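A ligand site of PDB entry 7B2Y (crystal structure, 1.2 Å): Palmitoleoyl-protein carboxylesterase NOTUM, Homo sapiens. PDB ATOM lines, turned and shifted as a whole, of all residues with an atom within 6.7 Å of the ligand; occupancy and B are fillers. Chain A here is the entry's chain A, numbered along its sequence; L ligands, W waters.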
ATOM      1  N   GLU A  48     -10.001  14.851  21.144  1.00  0.00           N
ATOM      2  CA  GLU A  48      -9.206  13.723  21.604  1.00  0.00           C
ATOM      3  C   GLU A  48      -7.729  14.109  21.601  1.00  0.00           C
ATOM      4  O   GLU A  48      -7.250  14.931  20.784  1.00  0.00           O
ATOM      5  CB  GLU A  48      -9.444  12.558  20.630  1.00  0.00           C
ATOM      6  CG  GLU A  48      -8.815  11.270  21.064  1.00  0.00           C
ATOM      7  CD  GLU A  48      -8.977  10.168  20.045  1.00  0.00           C
ATOM      8  OE1 GLU A  48      -9.183  10.388  18.869  1.00  0.00           O
ATOM      9  OE2 GLU A  48      -8.862   8.975  20.479  1.00  0.00           O
ATOM     10  N   GLY A  49      -6.967  13.459  22.486  1.00  0.00           N
ATOM     11  CA  GLY A  49      -5.525  13.580  22.500  1.00  0.00           C
ATOM     12  C   GLY A  49      -4.821  12.353  21.945  1.00  0.00           C
ATOM     13  O   GLY A  49      -5.415  11.486  21.292  1.00  0.00           O
ATOM     14  N   GLY A  50      -3.505  12.306  22.217  1.00  0.00           N
ATOM     15  CA  GLY A  50      -2.641  11.216  21.815  1.00  0.00           C
ATOM     16  C   GLY A  50      -1.299  11.627  21.227  1.00  0.00           C
ATOM     17  O   GLY A  50      -0.940  11.139  20.133  1.00  0.00           O
ATOM     18  N   TRP A  51      -0.550  12.468  21.910  1.00  0.00           N
ATOM     19  CA  TRP A  51       0.792  12.866  21.478  1.00  0.00           C
ATOM     20  C   TRP A  51       0.690  13.519  20.097  1.00  0.00           C
ATOM     21  O   TRP A  51      -0.206  14.361  19.875  1.00  0.00           O
ATOM     22  CB  TRP A  51       1.800  11.702  21.614  1.00  0.00           C
ATOM     23  CG  TRP A  51       1.972  11.278  23.045  1.00  0.00           C
ATOM     24  CD1 TRP A  51       1.273  10.325  23.686  1.00  0.00           C
ATOM     25  CD2 TRP A  51       2.931  11.804  23.970  1.00  0.00           C
ATOM     26  NE1 TRP A  51       1.732  10.229  25.006  1.00  0.00           N
ATOM     27  CE2 TRP A  51       2.732  11.130  25.196  1.00  0.00           C
ATOM     28  CE3 TRP A  51       3.914  12.784  23.897  1.00  0.00           C
ATOM     29  CZ2 TRP A  51       3.522  11.387  26.327  1.00  0.00           C
ATOM     30  CZ3 TRP A  51       4.694  13.076  25.041  1.00  0.00           C
ATOM     31  CH2 TRP A  51       4.492  12.350  26.229  1.00  0.00           C
ATOM     32  N   TYR A  52       1.622  13.223  19.190  1.00  0.00           N
ATOM     33  CA  TYR A  52       1.834  13.951  17.937  1.00  0.00           C
ATOM     34  C   TYR A  52       2.965  13.212  17.219  1.00  0.00           C
ATOM     35  O   TYR A  52       3.597  12.343  17.807  1.00  0.00           O
ATOM     36  CB  TYR A  52       2.205  15.435  18.152  1.00  0.00           C
ATOM     37  CG  TYR A  52       3.236  15.645  19.251  1.00  0.00           C
ATOM     38  CD1 TYR A  52       4.580  15.432  19.038  1.00  0.00           C
ATOM     39  CD2 TYR A  52       2.858  16.028  20.516  1.00  0.00           C
ATOM     40  CE1 TYR A  52       5.511  15.585  20.042  1.00  0.00           C
ATOM     41  CE2 TYR A  52       3.793  16.233  21.533  1.00  0.00           C
ATOM     42  CZ  TYR A  52       5.108  15.977  21.297  1.00  0.00           C
ATOM     43  OH  TYR A  52       5.981  16.160  22.356  1.00  0.00           O
ATOM     44  N   TYR A 105      -8.909  12.651  17.041  1.00  0.00           N
ATOM     45  CA  TYR A 105      -7.602  13.253  16.726  1.00  0.00           C
ATOM     46  C   TYR A 105      -6.938  12.383  15.676  1.00  0.00           C
ATOM     47  O   TYR A 105      -6.458  11.305  15.988  1.00  0.00           O
ATOM     48  CB  TYR A 105      -6.792  13.283  18.014  1.00  0.00           C
ATOM     49  CG  TYR A 105      -5.409  13.863  17.941  1.00  0.00           C
ATOM     50  CD1 TYR A 105      -5.125  15.046  17.254  1.00  0.00           C
ATOM     51  CD2 TYR A 105      -4.410  13.294  18.705  1.00  0.00           C
ATOM     52  CE1 TYR A 105      -3.844  15.586  17.273  1.00  0.00           C
ATOM     53  CE2 TYR A 105      -3.121  13.888  18.769  1.00  0.00           C
ATOM     54  CZ  TYR A 105      -2.856  15.014  18.044  1.00  0.00           C
ATOM     55  OH  TYR A 105      -1.618  15.580  18.073  1.00  0.00           O
ATOM     56  N   VAL A 110      -1.209  18.334  17.322  1.00  0.00           N
ATOM     57  CA  VAL A 110      -1.681  19.028  18.534  1.00  0.00           C
ATOM     58  C   VAL A 110      -2.809  19.990  18.067  1.00  0.00           C
ATOM     59  O   VAL A 110      -2.999  21.078  18.605  1.00  0.00           O
ATOM     60  CB  VAL A 110      -0.541  19.780  19.253  1.00  0.00           C
ATOM     61  CG1 VAL A 110      -1.008  20.273  20.636  1.00  0.00           C
ATOM     62  CG2 VAL A 110       0.698  18.937  19.314  1.00  0.00           C
ATOM     63  N   SER A 154      -8.380  16.672  25.966  1.00  0.00           N
ATOM     64  CA  SER A 154      -7.425  16.072  26.904  1.00  0.00           C
ATOM     65  C   SER A 154      -6.065  15.873  26.241  1.00  0.00           C
ATOM     66  O   SER A 154      -5.977  15.403  25.108  1.00  0.00           O
ATOM     67  CB  SER A 154      -7.951  14.724  27.446  1.00  0.00           C
ATOM     68  OG  SER A 154      -9.166  14.924  28.186  1.00  0.00           O
ATOM     69  N   SER A 155      -4.980  16.079  27.025  1.00  0.00           N
ATOM     70  CA  SER A 155      -3.583  15.870  26.590  1.00  0.00           C
ATOM     71  C   SER A 155      -3.353  16.771  25.392  1.00  0.00           C
ATOM     72  O   SER A 155      -3.574  17.978  25.503  1.00  0.00           O
ATOM     73  CB  SER A 155      -3.278  14.392  26.425  1.00  0.00           C
ATOM     74  OG  SER A 155      -1.843  14.248  26.405  1.00  0.00           O
ATOM     75  N   ALA A 156      -2.958  16.254  24.222  1.00  0.00           N
ATOM     76  CA  ALA A 156      -2.778  17.113  23.037  1.00  0.00           C
ATOM     77  C   ALA A 156      -4.074  17.822  22.678  1.00  0.00           C
ATOM     78  O   ALA A 156      -4.049  18.896  22.108  1.00  0.00           O
ATOM     79  CB  ALA A 156      -2.263  16.321  21.839  1.00  0.00           C
ATOM     80  N   GLY A 157      -5.227  17.201  22.985  1.00  0.00           N
ATOM     81  CA  GLY A 157      -6.491  17.890  22.775  1.00  0.00           C
ATOM     82  C   GLY A 157      -6.695  19.059  23.734  1.00  0.00           C
ATOM     83  O   GLY A 157      -7.333  20.067  23.363  1.00  0.00           O
ATOM     84  N   THR A 159      -4.143  20.951  24.920  1.00  0.00           N
ATOM     85  CA  THR A 159      -3.357  22.007  24.280  1.00  0.00           C
ATOM     86  C   THR A 159      -4.089  22.545  23.052  1.00  0.00           C
ATOM     87  O   THR A 159      -4.112  23.755  22.806  1.00  0.00           O
ATOM     88  CB  THR A 159      -1.968  21.483  23.937  1.00  0.00           C
ATOM     89  OG1 THR A 159      -1.425  20.772  25.060  1.00  0.00           O
ATOM     90  CG2 THR A 159      -1.044  22.628  23.506  1.00  0.00           C
ATOM     91  N   SER A 188      -5.165  18.364  31.072  1.00  0.00           N
ATOM     92  CA  SER A 188      -3.890  17.667  30.886  1.00  0.00           C
ATOM     93  C   SER A 188      -3.165  18.161  29.644  1.00  0.00           C
ATOM     94  O   SER A 188      -2.423  17.388  28.990  1.00  0.00           O
ATOM     95  CB  SER A 188      -4.111  16.164  30.843  1.00  0.00           C
ATOM     96  OG  SER A 188      -4.762  15.777  32.106  1.00  0.00           O
ATOM     97  N   GLY A 189      -3.325  19.416  29.296  1.00  0.00           N
ATOM     98  CA  GLY A 189      -2.642  20.047  28.175  1.00  0.00           C
ATOM     99  C   GLY A 189      -1.782  21.220  28.546  1.00  0.00           C
ATOM    100  O   GLY A 189      -1.426  22.025  27.665  1.00  0.00           O
ATOM    101  N   PHE A 191       1.597  22.120  29.867  1.00  0.00           N
ATOM    102  CA  PHE A 191       2.921  21.548  30.056  1.00  0.00           C
ATOM    103  C   PHE A 191       3.949  22.624  30.317  1.00  0.00           C
ATOM    104  O   PHE A 191       3.755  23.783  29.959  1.00  0.00           O
ATOM    105  CB  PHE A 191       3.311  20.738  28.819  1.00  0.00           C
ATOM    106  CG  PHE A 191       2.373  19.583  28.587  1.00  0.00           C
ATOM    107  CD1 PHE A 191       2.337  18.531  29.456  1.00  0.00           C
ATOM    108  CD2 PHE A 191       1.466  19.625  27.536  1.00  0.00           C
ATOM    109  CE1 PHE A 191       1.421  17.521  29.246  1.00  0.00           C
ATOM    110  CE2 PHE A 191       0.560  18.595  27.323  1.00  0.00           C
ATOM    111  CZ  PHE A 191       0.525  17.602  28.134  1.00  0.00           C
ATOM    112  N   PRO A 210      10.146  18.324  24.089  1.00  0.00           N
ATOM    113  CA  PRO A 210       8.969  18.914  23.418  1.00  0.00           C
ATOM    114  C   PRO A 210       9.205  20.267  22.815  1.00  0.00           C
ATOM    115  O   PRO A 210       8.694  20.520  21.725  1.00  0.00           O
ATOM    116  CB  PRO A 210       7.916  18.984  24.542  1.00  0.00           C
ATOM    117  CG  PRO A 210       8.293  17.818  25.392  1.00  0.00           C
ATOM    118  CD  PRO A 210       9.802  17.811  25.434  1.00  0.00           C
ATOM    119  N   THR A 211      10.044  21.123  23.416  1.00  0.00           N
ATOM    120  CA  THR A 211      10.291  22.399  22.760  1.00  0.00           C
ATOM    121  C   THR A 211      10.902  22.199  21.382  1.00  0.00           C
ATOM    122  O   THR A 211      10.484  22.870  20.438  1.00  0.00           O
ATOM    123  CB  THR A 211      11.182  23.329  23.577  1.00  0.00           C
ATOM    124  OG1 THR A 211      12.420  22.707  23.827  1.00  0.00           O
ATOM    125  CG2 THR A 211      10.537  23.739  24.905  1.00  0.00           C
ATOM    126  N   ILE A 214       8.278  20.291  18.990  1.00  0.00           N
ATOM    127  CA  ILE A 214       7.234  21.223  18.548  1.00  0.00           C
ATOM    128  C   ILE A 214       7.784  22.267  17.581  1.00  0.00           C
ATOM    129  O   ILE A 214       7.149  22.591  16.566  1.00  0.00           O
ATOM    130  CB  ILE A 214       6.585  21.880  19.779  1.00  0.00           C
ATOM    131  CG1 ILE A 214       5.810  20.873  20.640  1.00  0.00           C
ATOM    132  CG2 ILE A 214       5.639  23.028  19.360  1.00  0.00           C
ATOM    133  CD1 ILE A 214       4.637  20.201  20.033  1.00  0.00           C
ATOM    134  N   PHE A 242       2.571  26.740  22.404  1.00  0.00           N
ATOM    135  CA  PHE A 242       2.083  25.421  22.764  1.00  0.00           C
ATOM    136  C   PHE A 242       2.208  25.169  24.254  1.00  0.00           C
ATOM    137  O   PHE A 242       1.768  24.105  24.721  1.00  0.00           O
ATOM    138  CB  PHE A 242       2.844  24.346  21.996  1.00  0.00           C
ATOM    139  CG  PHE A 242       2.413  24.199  20.545  1.00  0.00           C
ATOM    140  CD1 PHE A 242       2.631  25.224  19.629  1.00  0.00           C
ATOM    141  CD2 PHE A 242       1.922  22.981  20.076  1.00  0.00           C
ATOM    142  CE1 PHE A 242       2.268  25.051  18.271  1.00  0.00           C
ATOM    143  CE2 PHE A 242       1.580  22.843  18.711  1.00  0.00           C
ATOM    144  CZ  PHE A 242       1.742  23.840  17.857  1.00  0.00           C
ATOM    145  N   PHE A 243       2.764  26.115  25.012  1.00  0.00           N
ATOM    146  CA  PHE A 243       2.942  25.970  26.452  1.00  0.00           C
ATOM    147  C   PHE A 243       1.912  26.831  27.148  1.00  0.00           C
ATOM    148  O   PHE A 243       1.923  28.051  27.010  1.00  0.00           O
ATOM    149  CB  PHE A 243       4.397  26.288  26.828  1.00  0.00           C
ATOM    150  CG  PHE A 243       5.306  25.209  26.313  1.00  0.00           C
ATOM    151  CD1 PHE A 243       5.534  24.085  27.069  1.00  0.00           C
ATOM    152  CD2 PHE A 243       5.799  25.242  25.028  1.00  0.00           C
ATOM    153  CE1 PHE A 243       6.274  23.014  26.549  1.00  0.00           C
ATOM    154  CE2 PHE A 243       6.524  24.204  24.511  1.00  0.00           C
ATOM    155  CZ  PHE A 243       6.738  23.084  25.287  1.00  0.00           C
ATOM    156  N   ASP A 263       1.760  15.400  36.231  1.00  0.00           N
ATOM    157  CA  ASP A 263       1.198  14.726  35.065  1.00  0.00           C
ATOM    158  C   ASP A 263       2.184  13.703  34.518  1.00  0.00           C
ATOM    159  O   ASP A 263       3.380  14.008  34.356  1.00  0.00           O
ATOM    160  CB  ASP A 263       0.847  15.787  34.016  1.00  0.00           C
ATOM    161  CG  ASP A 263       0.180  15.218  32.861  1.00  0.00           C
ATOM    162  OD1 ASP A 263      -1.025  15.077  32.848  1.00  0.00           O
ATOM    163  OD2 ASP A 263       0.941  14.877  31.912  1.00  0.00           O
ATOM    164  N   ALA A 265       2.606  12.468  31.560  1.00  0.00           N
ATOM    165  CA  ALA A 265       3.227  12.877  30.312  1.00  0.00           C
ATOM    166  C   ALA A 265       4.290  13.947  30.518  1.00  0.00           C
ATOM    167  O   ALA A 265       5.344  13.918  29.847  1.00  0.00           O
ATOM    168  CB  ALA A 265       2.155  13.337  29.339  1.00  0.00           C
ATOM    169  N   GLN A 266       4.082  14.881  31.458  1.00  0.00           N
ATOM    170  CA  GLN A 266       5.124  15.838  31.814  1.00  0.00           C
ATOM    171  C   GLN A 266       6.335  15.110  32.380  1.00  0.00           C
ATOM    172  O   GLN A 266       7.476  15.361  31.965  1.00  0.00           O
ATOM    173  CB  GLN A 266       4.587  16.791  32.868  1.00  0.00           C
ATOM    174  CG  GLN A 266       5.624  17.813  33.333  1.00  0.00           C
ATOM    175  CD  GLN A 266       5.848  18.926  32.328  1.00  0.00           C
ATOM    176  OE1 GLN A 266       4.896  19.554  31.845  1.00  0.00           O
ATOM    177  NE2 GLN A 266       7.127  19.163  31.974  1.00  0.00           N
ATOM    178  N   VAL A 269       8.304  13.424  29.456  1.00  0.00           N
ATOM    179  CA  VAL A 269       9.124  14.312  28.646  1.00  0.00           C
ATOM    180  C   VAL A 269      10.252  14.930  29.454  1.00  0.00           C
ATOM    181  O   VAL A 269      11.243  15.382  28.872  1.00  0.00           O
ATOM    182  CB  VAL A 269       8.316  15.390  27.906  1.00  0.00           C
ATOM    183  CG1 VAL A 269       7.278  14.750  26.988  1.00  0.00           C
ATOM    184  CG2 VAL A 269       7.666  16.357  28.897  1.00  0.00           C
ATOM    185  N   HIS A 312      -2.938  11.173  34.502  1.00  0.00           N
ATOM    186  CA  HIS A 312      -2.921  11.747  33.156  1.00  0.00           C
ATOM    187  C   HIS A 312      -4.336  11.723  32.624  1.00  0.00           C
ATOM    188  O   HIS A 312      -4.914  10.632  32.494  1.00  0.00           O
ATOM    189  CB  HIS A 312      -1.994  10.939  32.230  1.00  0.00           C
ATOM    190  CG  HIS A 312      -1.871  11.511  30.833  1.00  0.00           C
ATOM    191  ND1 HIS A 312      -1.456  12.805  30.603  1.00  0.00           N
ATOM    192  CD2 HIS A 312      -2.128  10.959  29.627  1.00  0.00           C
ATOM    193  CE1 HIS A 312      -1.459  13.032  29.291  1.00  0.00           C
ATOM    194  NE2 HIS A 312      -1.854  11.932  28.685  1.00  0.00           N
ATOM    195  N   GLU A 313      -4.873  12.889  32.285  1.00  0.00           N
ATOM    196  CA  GLU A 313      -6.236  13.126  31.773  1.00  0.00           C
ATOM    197  C   GLU A 313      -7.233  12.860  32.883  1.00  0.00           C
ATOM    198  O   GLU A 313      -6.906  12.209  33.879  1.00  0.00           O
ATOM    199  CB  GLU A 313      -6.536  12.314  30.507  1.00  0.00           C
ATOM    200  CG  GLU A 313      -5.491  12.504  29.416  1.00  0.00           C
ATOM    201  CD  GLU A 313      -5.823  11.743  28.172  1.00  0.00           C
ATOM    202  OE1 GLU A 313      -5.708  12.338  27.105  1.00  0.00           O
ATOM    203  OE2 GLU A 313      -6.165  10.546  28.247  1.00  0.00           O
HETATM  204  C1  LIG L   1      -1.267  13.662  25.301  1.00  0.00           C
HETATM  205  C2  LIG L   1       0.165  13.264  25.538  1.00  0.00           C
HETATM  206  C3  LIG L   1       1.090  14.338  26.051  1.00  0.00           C
HETATM  207  C4  LIG L   1       1.134  15.530  25.130  1.00  0.00           C
HETATM  208  C5  LIG L   1       3.244  16.294  26.275  1.00  0.00           C
HETATM  209  C6  LIG L   1       4.240  17.393  26.056  1.00  0.00           C
HETATM  210  C7  LIG L   1       3.516  18.345  25.133  1.00  0.00           C
HETATM  211  C8  LIG L   1       3.847  19.645  24.776  1.00  0.00           C
HETATM  212  C9  LIG L   1       2.956  20.321  23.940  1.00  0.00           C
HETATM  213  C10 LIG L   1       1.784  19.702  23.502  1.00  0.00           C
HETATM  214  C11 LIG L   1       1.451  18.394  23.838  1.00  0.00           C
HETATM  215  C12 LIG L   1       2.370  17.725  24.667  1.00  0.00           C
HETATM  216  N1  LIG L   1       2.192  16.445  25.281  1.00  0.00           N
HETATM  217  O1  LIG L   1      -1.845  13.533  24.280  1.00  0.00           O
HETATM  218  O2  LIG L   1       0.278  15.770  24.299  1.00  0.00           O
HETATM  219  O   HOH W   1      -2.135  11.112  26.168  1.00  0.00           O
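OG of Ser 155 is covalently linked to C1 of the ligand. An oxygen (O1) of the ligand lies within hydrogen-bond range of the backbone NH (N) of Ala 156, 2.9 Å away. The backbone NH (N) of Trp 51 is in hydrogen-bond range of an oxygen (O1) of the ligand (2.9 Å). N of Gly 50 lies within hydrogen-bond range of O1 of the ligand, at 2.9 Å.
ND1 of His 312 is in hydrogen-bond range of OD1 of Asp 263, at 3.2 Å. N of Ala 265 lies within hydrogen-bond range of OD2 of Asp 263 (2.9 Å). The backbone carbonyl oxygen of Ser 188 sits close to the backbone NH of Ser 155. The side-chain hydroxyl (OH) of Tyr 105 sits at hydrogen-bond distance from the backbone carbonyl oxygen (O) of Trp 51, 2.6 Å away. The side-chain hydroxyl of Thr 159 is in hydrogen-bond range of the backbone carbonyl oxygen of Gly 189 (2.9 Å). A ring nitrogen (NE2) of His 312 sits close to the side-chain hydroxyl of Ser 155 (3.2 Å). O of Ser 154 lies close to N of Gly 49 (3.4 Å).
Residues that only touch the ligand: Gly 49 (3.96 Å), Tyr 52 (3.8 Å), Thr 159 (3.7 Å), Phe 191 (3.3 Å), Ala 265 (3.6 Å) and His 312 (3.8 Å). Within 4 Å of the ligand: Gly 49, Gly 50, Trp 51, Tyr 52, Ser 155, Ala 156, Thr 159, Phe 191, Ala 265 and His 312. Along chain A the residues within 4 Å of the ligand span positions 49 to 312.
Water W1 lies within hydrogen-bond range of NE2 of His 312 (2.7 Å), O1 of the ligand (3.1 Å) and OG of Ser 155 (3.2 Å).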
